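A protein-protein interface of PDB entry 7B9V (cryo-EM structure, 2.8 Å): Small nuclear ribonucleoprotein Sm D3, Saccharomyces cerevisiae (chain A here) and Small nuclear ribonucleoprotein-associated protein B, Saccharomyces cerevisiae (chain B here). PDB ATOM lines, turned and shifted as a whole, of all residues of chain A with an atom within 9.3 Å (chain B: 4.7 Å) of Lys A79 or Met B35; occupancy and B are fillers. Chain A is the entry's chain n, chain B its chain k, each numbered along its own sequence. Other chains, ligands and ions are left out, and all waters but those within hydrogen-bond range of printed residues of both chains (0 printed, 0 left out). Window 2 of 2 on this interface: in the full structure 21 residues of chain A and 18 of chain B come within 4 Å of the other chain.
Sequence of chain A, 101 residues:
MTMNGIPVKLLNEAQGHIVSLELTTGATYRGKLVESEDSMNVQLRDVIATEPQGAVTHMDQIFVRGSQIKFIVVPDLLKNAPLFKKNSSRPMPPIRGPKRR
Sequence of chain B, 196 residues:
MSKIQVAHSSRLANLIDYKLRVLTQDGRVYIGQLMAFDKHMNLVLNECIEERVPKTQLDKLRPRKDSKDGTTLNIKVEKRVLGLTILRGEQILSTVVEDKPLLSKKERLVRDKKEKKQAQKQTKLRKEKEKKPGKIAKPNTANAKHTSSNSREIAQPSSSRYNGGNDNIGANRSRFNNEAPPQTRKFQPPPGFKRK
O of Gln B33 sits at hydrogen-bond distance from N of Asn B46, 2.8 Å away. N of Met B35 lies within hydrogen-bond range of O of Val B44, at 3.0 Å. The backbone carbonyl oxygen of Ala B36 is in hydrogen-bond range of the backbone NH of Val B44 (3.0 Å). The side-chain amino group (NZ) of Lys A79 lies within salt-bridge range of the side-chain carboxylate (OD2) of Asp A76 (2.7 Å).
Ala B36 touches Ile A6. Val B44 touches Pro A7. Val B44 touches Leu A10. Leu B84 touches Val A74 (O to CB, 3.6 Å). Asp A76 touches Asn B46 (OD1 to OD1, 3.7 Å). CB of Leu A78 touches CD2 of Leu B84, 3.7 Å away. O of Lys A79 touches CE of Met B35, at 3.7 Å. Lys A79 touches Asn B46. Lys A79 touches Leu B84. Met B35 touches Phe A84 (CE to CD2, 3.6 Å).
Of the printed residues of chain B, Ile A6 touches Ala B36. Glu A13 touches none of the printed residues of chain B. Printed residues of chain B within 4 Å of Pro A75: Leu B84 (3.7 Å). Printed residues of chain B within 4 Å of Lys A79: Met B35, Asn B46 and Leu B84. Lys A86 touches none of the printed residues of chain B. Met B35 touches just these residues of chain A: Lys A79 (3.7 Å) and Phe A84 (3.6 Å). Ala B36 touches one residue of chain A. The nearest printed residue of chain B that does not touch Lys A79 is Val B44 (7.9 Å). The nearest residue of chain A that does not touch Met B35 is Leu A78 (5.6 Å).
Of the 8 printed residues of chain B, 5 touch a printed residue of chain A. Along chain B the printed residues that touch a printed residue of chain A span positions 35 to 84. Of the 17 printed residues of chain A, 9 touch a printed residue of chain B. Hydrophobic or aromatic side chains of chain A within 4 Å of the printed part of chain B: Ile A6, Pro A7, Leu A10, Val A74, Leu A78 and Phe A84. Along chain A the printed residues that touch a printed residue of chain B span positions 6 to 84. Among the printed residues, 11 pairs touch across the chains. Among the printed residues, no Asp or Glu carboxylate lies within 4 Å of a Lys or Arg side-chain nitrogen of the other chain.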
ATOM      1  N   ILE A   6     -26.505  -2.448  14.574  1.00  0.00           N
ATOM      2  CA  ILE A   6     -26.282  -3.560  15.529  1.00  0.00           C
ATOM      3  C   ILE A   6     -26.703  -3.242  16.971  1.00  0.00           C
ATOM      4  O   ILE A   6     -27.377  -4.082  17.577  1.00  0.00           O
ATOM      5  CB  ILE A   6     -24.840  -4.068  15.402  1.00  0.00           C
ATOM      6  CG1 ILE A   6     -24.716  -4.876  14.120  1.00  0.00           C
ATOM      7  CG2 ILE A   6     -24.551  -5.137  16.434  1.00  0.00           C
ATOM      8  CD1 ILE A   6     -23.329  -5.433  13.825  1.00  0.00           C
ATOM      9  N   PRO A   7     -26.472  -1.973  17.563  1.00  0.00           N
ATOM     10  CA  PRO A   7     -26.932  -1.673  18.947  1.00  0.00           C
ATOM     11  C   PRO A   7     -28.447  -1.690  19.217  1.00  0.00           C
ATOM     12  O   PRO A   7     -28.887  -1.382  20.329  1.00  0.00           O
ATOM     13  CB  PRO A   7     -26.326  -0.307  19.283  1.00  0.00           C
ATOM     14  CG  PRO A   7     -25.142  -0.258  18.508  1.00  0.00           C
ATOM     15  CD  PRO A   7     -25.556  -0.875  17.199  1.00  0.00           C
ATOM     16  N   LEU A  10     -29.234  -6.053  18.380  1.00  0.00           N
ATOM     17  CA  LEU A  10     -28.862  -6.745  19.617  1.00  0.00           C
ATOM     18  C   LEU A  10     -30.003  -6.772  20.602  1.00  0.00           C
ATOM     19  O   LEU A  10     -30.328  -7.837  21.139  1.00  0.00           O
ATOM     20  CB  LEU A  10     -27.617  -6.096  20.230  1.00  0.00           C
ATOM     21  CG  LEU A  10     -27.089  -6.668  21.543  1.00  0.00           C
ATOM     22  CD1 LEU A  10     -26.623  -8.095  21.351  1.00  0.00           C
ATOM     23  CD2 LEU A  10     -25.959  -5.822  22.071  1.00  0.00           C
ATOM     24  N   GLU A  13     -32.425  -9.132  19.667  1.00  0.00           N
ATOM     25  CA  GLU A  13     -32.037 -10.525  19.910  1.00  0.00           C
ATOM     26  C   GLU A  13     -32.128 -10.910  21.394  1.00  0.00           C
ATOM     27  O   GLU A  13     -32.362 -12.084  21.717  1.00  0.00           O
ATOM     28  CB  GLU A  13     -30.629 -10.808  19.343  1.00  0.00           C
ATOM     29  CG  GLU A  13     -29.963 -12.201  19.633  1.00  0.00           C
ATOM     30  CD  GLU A  13     -30.801 -13.477  19.340  1.00  0.00           C
ATOM     31  OE1 GLU A  13     -31.809 -13.460  18.597  1.00  0.00           O
ATOM     32  OE2 GLU A  13     -30.467 -14.526  19.934  1.00  0.00           O
ATOM     33  N   VAL A  74     -27.118  -6.945  29.099  1.00  0.00           N
ATOM     34  CA  VAL A  74     -27.644  -8.049  28.303  1.00  0.00           C
ATOM     35  C   VAL A  74     -26.921  -9.324  28.744  1.00  0.00           C
ATOM     36  O   VAL A  74     -25.859  -9.185  29.369  1.00  0.00           O
ATOM     37  CB  VAL A  74     -27.396  -7.670  26.820  1.00  0.00           C
ATOM     38  CG1 VAL A  74     -27.700  -8.706  25.820  1.00  0.00           C
ATOM     39  CG2 VAL A  74     -28.263  -6.462  26.417  1.00  0.00           C
ATOM     40  N   PRO A  75     -27.513 -10.527  28.657  1.00  0.00           N
ATOM     41  CA  PRO A  75     -26.747 -11.763  28.947  1.00  0.00           C
ATOM     42  C   PRO A  75     -25.460 -11.874  28.129  1.00  0.00           C
ATOM     43  O   PRO A  75     -25.452 -11.595  26.932  1.00  0.00           O
ATOM     44  CB  PRO A  75     -27.743 -12.902  28.660  1.00  0.00           C
ATOM     45  CG  PRO A  75     -28.856 -12.313  27.915  1.00  0.00           C
ATOM     46  CD  PRO A  75     -28.910 -10.870  28.413  1.00  0.00           C
ATOM     47  N   ASP A  76     -24.353 -12.243  28.801  1.00  0.00           N
ATOM     48  CA  ASP A  76     -23.033 -12.386  28.156  1.00  0.00           C
ATOM     49  C   ASP A  76     -22.999 -13.391  26.993  1.00  0.00           C
ATOM     50  O   ASP A  76     -22.070 -13.348  26.178  1.00  0.00           O
ATOM     51  CB  ASP A  76     -22.010 -12.760  29.236  1.00  0.00           C
ATOM     52  CG  ASP A  76     -20.572 -12.621  28.771  1.00  0.00           C
ATOM     53  OD1 ASP A  76     -20.041 -11.491  28.793  1.00  0.00           O
ATOM     54  OD2 ASP A  76     -19.976 -13.647  28.394  1.00  0.00           O
ATOM     55  N   LEU A  77     -24.000 -14.280  26.897  1.00  0.00           N
ATOM     56  CA  LEU A  77     -24.108 -15.304  25.861  1.00  0.00           C
ATOM     57  C   LEU A  77     -24.261 -14.711  24.468  1.00  0.00           C
ATOM     58  O   LEU A  77     -23.931 -15.379  23.481  1.00  0.00           O
ATOM     59  CB  LEU A  77     -25.321 -16.185  26.137  1.00  0.00           C
ATOM     60  CG  LEU A  77     -25.419 -16.860  27.500  1.00  0.00           C
ATOM     61  CD1 LEU A  77     -26.806 -17.475  27.676  1.00  0.00           C
ATOM     62  CD2 LEU A  77     -24.335 -17.906  27.631  1.00  0.00           C
ATOM     63  N   LEU A  78     -24.753 -13.483  24.368  1.00  0.00           N
ATOM     64  CA  LEU A  78     -25.025 -12.858  23.080  1.00  0.00           C
ATOM     65  C   LEU A  78     -23.774 -12.381  22.348  1.00  0.00           C
ATOM     66  O   LEU A  78     -23.911 -11.895  21.223  1.00  0.00           O
ATOM     67  CB  LEU A  78     -26.091 -11.758  23.220  1.00  0.00           C
ATOM     68  CG  LEU A  78     -27.559 -12.249  23.067  1.00  0.00           C
ATOM     69  CD1 LEU A  78     -28.036 -13.457  23.887  1.00  0.00           C
ATOM     70  CD2 LEU A  78     -28.568 -11.116  23.205  1.00  0.00           C
ATOM     71  N   LYS A  79     -22.590 -12.390  22.982  1.00  0.00           N
ATOM     72  CA  LYS A  79     -21.359 -11.981  22.295  1.00  0.00           C
ATOM     73  C   LYS A  79     -21.014 -12.892  21.106  1.00  0.00           C
ATOM     74  O   LYS A  79     -20.257 -12.481  20.219  1.00  0.00           O
ATOM     75  CB  LYS A  79     -20.186 -11.932  23.280  1.00  0.00           C
ATOM     76  CG  LYS A  79     -19.731 -13.296  23.808  1.00  0.00           C
ATOM     77  CD  LYS A  79     -18.842 -13.161  25.040  1.00  0.00           C
ATOM     78  CE  LYS A  79     -18.455 -14.525  25.590  1.00  0.00           C
ATOM     79  NZ  LYS A  79     -17.869 -14.409  26.955  1.00  0.00           N
ATOM     80  N   ASN A  80     -21.550 -14.114  21.080  1.00  0.00           N
ATOM     81  CA  ASN A  80     -21.377 -15.060  19.989  1.00  0.00           C
ATOM     82  C   ASN A  80     -22.658 -15.288  19.194  1.00  0.00           C
ATOM     83  O   ASN A  80     -22.737 -16.265  18.443  1.00  0.00           O
ATOM     84  CB  ASN A  80     -20.859 -16.388  20.534  1.00  0.00           C
ATOM     85  CG  ASN A  80     -19.465 -16.276  21.098  1.00  0.00           C
ATOM     86  OD1 ASN A  80     -19.270 -16.354  22.310  1.00  0.00           O
ATOM     87  ND2 ASN A  80     -18.484 -16.072  20.228  1.00  0.00           N
ATOM     88  N   ALA A  81     -23.673 -14.436  19.361  1.00  0.00           N
ATOM     89  CA  ALA A  81     -24.870 -14.446  18.513  1.00  0.00           C
ATOM     90  C   ALA A  81     -24.488 -14.129  17.058  1.00  0.00           C
ATOM     91  O   ALA A  81     -23.451 -13.496  16.833  1.00  0.00           O
ATOM     92  CB  ALA A  81     -25.873 -13.423  19.060  1.00  0.00           C
ATOM     93  N   PRO A  82     -25.281 -14.571  16.051  1.00  0.00           N
ATOM     94  CA  PRO A  82     -24.867 -14.373  14.637  1.00  0.00           C
ATOM     95  C   PRO A  82     -24.732 -12.918  14.210  1.00  0.00           C
ATOM     96  O   PRO A  82     -24.079 -12.643  13.195  1.00  0.00           O
ATOM     97  CB  PRO A  82     -25.951 -15.105  13.817  1.00  0.00           C
ATOM     98  CG  PRO A  82     -27.135 -15.124  14.655  1.00  0.00           C
ATOM     99  CD  PRO A  82     -26.560 -15.285  16.074  1.00  0.00           C
ATOM    100  N   LEU A  83     -25.417 -12.035  14.935  1.00  0.00           N
ATOM    101  CA  LEU A  83     -25.512 -10.598  14.714  1.00  0.00           C
ATOM    102  C   LEU A  83     -24.194  -9.899  14.405  1.00  0.00           C
ATOM    103  O   LEU A  83     -24.108  -9.075  13.484  1.00  0.00           O
ATOM    104  CB  LEU A  83     -26.070 -10.003  15.987  1.00  0.00           C
ATOM    105  CG  LEU A  83     -26.177  -8.511  15.918  1.00  0.00           C
ATOM    106  CD1 LEU A  83     -27.186  -8.129  14.837  1.00  0.00           C
ATOM    107  CD2 LEU A  83     -26.553  -8.123  17.252  1.00  0.00           C
ATOM    108  N   PHE A  84     -23.148 -10.274  15.120  1.00  0.00           N
ATOM    109  CA  PHE A  84     -21.869  -9.604  15.006  1.00  0.00           C
ATOM    110  C   PHE A  84     -21.026 -10.072  13.835  1.00  0.00           C
ATOM    111  O   PHE A  84     -19.949  -9.501  13.645  1.00  0.00           O
ATOM    112  CB  PHE A  84     -21.083  -9.749  16.315  1.00  0.00           C
ATOM    113  CG  PHE A  84     -21.727  -9.067  17.501  1.00  0.00           C
ATOM    114  CD1 PHE A  84     -21.743  -7.679  17.561  1.00  0.00           C
ATOM    115  CD2 PHE A  84     -22.349  -9.788  18.509  1.00  0.00           C
ATOM    116  CE1 PHE A  84     -22.322  -7.018  18.632  1.00  0.00           C
ATOM    117  CE2 PHE A  84     -22.945  -9.130  19.580  1.00  0.00           C
ATOM    118  CZ  PHE A  84     -22.930  -7.745  19.636  1.00  0.00           C
ATOM    119  N   LYS A  85     -21.434 -11.117  13.113  1.00  0.00           N
ATOM    120  CA  LYS A  85     -20.622 -11.651  12.024  1.00  0.00           C
ATOM    121  C   LYS A  85     -20.504 -10.643  10.877  1.00  0.00           C
ATOM    122  O   LYS A  85     -21.368  -9.782  10.682  1.00  0.00           O
ATOM    123  CB  LYS A  85     -21.206 -12.958  11.489  1.00  0.00           C
ATOM    124  CG  LYS A  85     -21.048 -14.142  12.421  1.00  0.00           C
ATOM    125  CD  LYS A  85     -21.678 -15.398  11.841  1.00  0.00           C
ATOM    126  CE  LYS A  85     -21.429 -16.597  12.743  1.00  0.00           C
ATOM    127  NZ  LYS A  85     -19.993 -17.007  12.728  1.00  0.00           N
ATOM    128  N   LYS A  86     -19.411 -10.754  10.126  1.00  0.00           N
ATOM    129  CA  LYS A  86     -19.177  -9.895   8.968  1.00  0.00           C
ATOM    130  C   LYS A  86     -20.143 -10.207   7.826  1.00  0.00           C
ATOM    131  O   LYS A  86     -19.970 -11.191   7.107  1.00  0.00           O
ATOM    132  CB  LYS A  86     -17.732 -10.030   8.475  1.00  0.00           C
ATOM    133  CG  LYS A  86     -16.670  -9.675   9.513  1.00  0.00           C
ATOM    134  CD  LYS A  86     -16.658  -8.185   9.840  1.00  0.00           C
ATOM    135  CE  LYS A  86     -15.525  -7.840  10.800  1.00  0.00           C
ATOM    136  NZ  LYS A  86     -15.697  -8.462  12.143  1.00  0.00           N
ATOM    137  N   ILE B  16     -13.089  -0.882  16.725  1.00  0.00           N
ATOM    138  CA  ILE B  16     -13.697  -2.158  17.094  1.00  0.00           C
ATOM    139  C   ILE B  16     -12.645  -3.034  17.766  1.00  0.00           C
ATOM    140  O   ILE B  16     -11.480  -3.064  17.334  1.00  0.00           O
ATOM    141  CB  ILE B  16     -14.280  -2.824  15.829  1.00  0.00           C
ATOM    142  CG1 ILE B  16     -15.475  -2.035  15.288  1.00  0.00           C
ATOM    143  CG2 ILE B  16     -14.699  -4.291  16.046  1.00  0.00           C
ATOM    144  CD1 ILE B  16     -16.666  -2.021  16.202  1.00  0.00           C
ATOM    145  N   GLN B  33     -14.585  -3.452  25.921  1.00  0.00           N
ATOM    146  CA  GLN B  33     -14.247  -3.689  24.523  1.00  0.00           C
ATOM    147  C   GLN B  33     -15.402  -3.285  23.620  1.00  0.00           C
ATOM    148  O   GLN B  33     -16.512  -3.811  23.754  1.00  0.00           O
ATOM    149  CB  GLN B  33     -13.918  -5.163  24.301  1.00  0.00           C
ATOM    150  CG  GLN B  33     -12.561  -5.617  24.811  1.00  0.00           C
ATOM    151  CD  GLN B  33     -12.159  -6.968  24.252  1.00  0.00           C
ATOM    152  OE1 GLN B  33     -12.426  -7.273  23.090  1.00  0.00           O
ATOM    153  NE2 GLN B  33     -11.496  -7.778  25.069  1.00  0.00           N
ATOM    154  N   LEU B  34     -15.137  -2.352  22.700  1.00  0.00           N
ATOM    155  CA  LEU B  34     -16.145  -1.927  21.740  1.00  0.00           C
ATOM    156  C   LEU B  34     -16.414  -3.044  20.746  1.00  0.00           C
ATOM    157  O   LEU B  34     -15.523  -3.456  19.996  1.00  0.00           O
ATOM    158  CB  LEU B  34     -15.680  -0.671  21.010  1.00  0.00           C
ATOM    159  CG  LEU B  34     -16.682  -0.041  20.047  1.00  0.00           C
ATOM    160  CD1 LEU B  34     -17.767   0.619  20.822  1.00  0.00           C
ATOM    161  CD2 LEU B  34     -15.998   0.978  19.152  1.00  0.00           C
ATOM    162  N   MET B  35     -17.653  -3.529  20.737  1.00  0.00           N
ATOM    163  CA  MET B  35     -18.087  -4.528  19.776  1.00  0.00           C
ATOM    164  C   MET B  35     -18.797  -3.935  18.571  1.00  0.00           C
ATOM    165  O   MET B  35     -18.599  -4.413  17.451  1.00  0.00           O
ATOM    166  CB  MET B  35     -19.018  -5.539  20.437  1.00  0.00           C
ATOM    167  CG  MET B  35     -18.305  -6.538  21.302  1.00  0.00           C
ATOM    168  SD  MET B  35     -19.349  -7.915  21.779  1.00  0.00           S
ATOM    169  CE  MET B  35     -19.316  -8.896  20.282  1.00  0.00           C
ATOM    170  N   ALA B  36     -19.620  -2.907  18.789  1.00  0.00           N
ATOM    171  CA  ALA B  36     -20.417  -2.305  17.733  1.00  0.00           C
ATOM    172  C   ALA B  36     -20.918  -0.939  18.143  1.00  0.00           C
ATOM    173  O   ALA B  36     -20.919  -0.582  19.323  1.00  0.00           O
ATOM    174  CB  ALA B  36     -21.616  -3.166  17.368  1.00  0.00           C
ATOM    175  N   VAL B  44     -22.032  -0.474  22.143  1.00  0.00           N
ATOM    176  CA  VAL B  44     -22.078  -1.798  22.751  1.00  0.00           C
ATOM    177  C   VAL B  44     -20.696  -2.207  23.232  1.00  0.00           C
ATOM    178  O   VAL B  44     -19.752  -2.315  22.439  1.00  0.00           O
ATOM    179  CB  VAL B  44     -22.610  -2.840  21.761  1.00  0.00           C
ATOM    180  CG1 VAL B  44     -22.567  -4.218  22.378  1.00  0.00           C
ATOM    181  CG2 VAL B  44     -24.016  -2.486  21.334  1.00  0.00           C
ATOM    182  N   ASN B  46     -18.502  -4.997  25.359  1.00  0.00           N
ATOM    183  CA  ASN B  46     -18.336  -6.297  25.984  1.00  0.00           C
ATOM    184  C   ASN B  46     -17.459  -6.124  27.203  1.00  0.00           C
ATOM    185  O   ASN B  46     -16.698  -5.153  27.277  1.00  0.00           O
ATOM    186  CB  ASN B  46     -17.672  -7.283  25.012  1.00  0.00           C
ATOM    187  CG  ASN B  46     -17.796  -8.731  25.456  1.00  0.00           C
ATOM    188  OD1 ASN B  46     -18.491  -9.037  26.423  1.00  0.00           O
ATOM    189  ND2 ASN B  46     -17.075  -9.619  24.783  1.00  0.00           N
ATOM    190  N   LEU B  84     -21.948  -7.017  28.646  1.00  0.00           N
ATOM    191  CA  LEU B  84     -22.418  -6.689  27.271  1.00  0.00           C
ATOM    192  C   LEU B  84     -23.378  -5.486  27.204  1.00  0.00           C
ATOM    193  O   LEU B  84     -24.514  -5.599  26.729  1.00  0.00           O
ATOM    194  CB  LEU B  84     -22.986  -7.937  26.585  1.00  0.00           C
ATOM    195  CG  LEU B  84     -23.160  -7.945  25.049  1.00  0.00           C
ATOM    196  CD1 LEU B  84     -21.790  -7.826  24.457  1.00  0.00           C
ATOM    197  CD2 LEU B  84     -23.776  -9.225  24.593  1.00  0.00           C
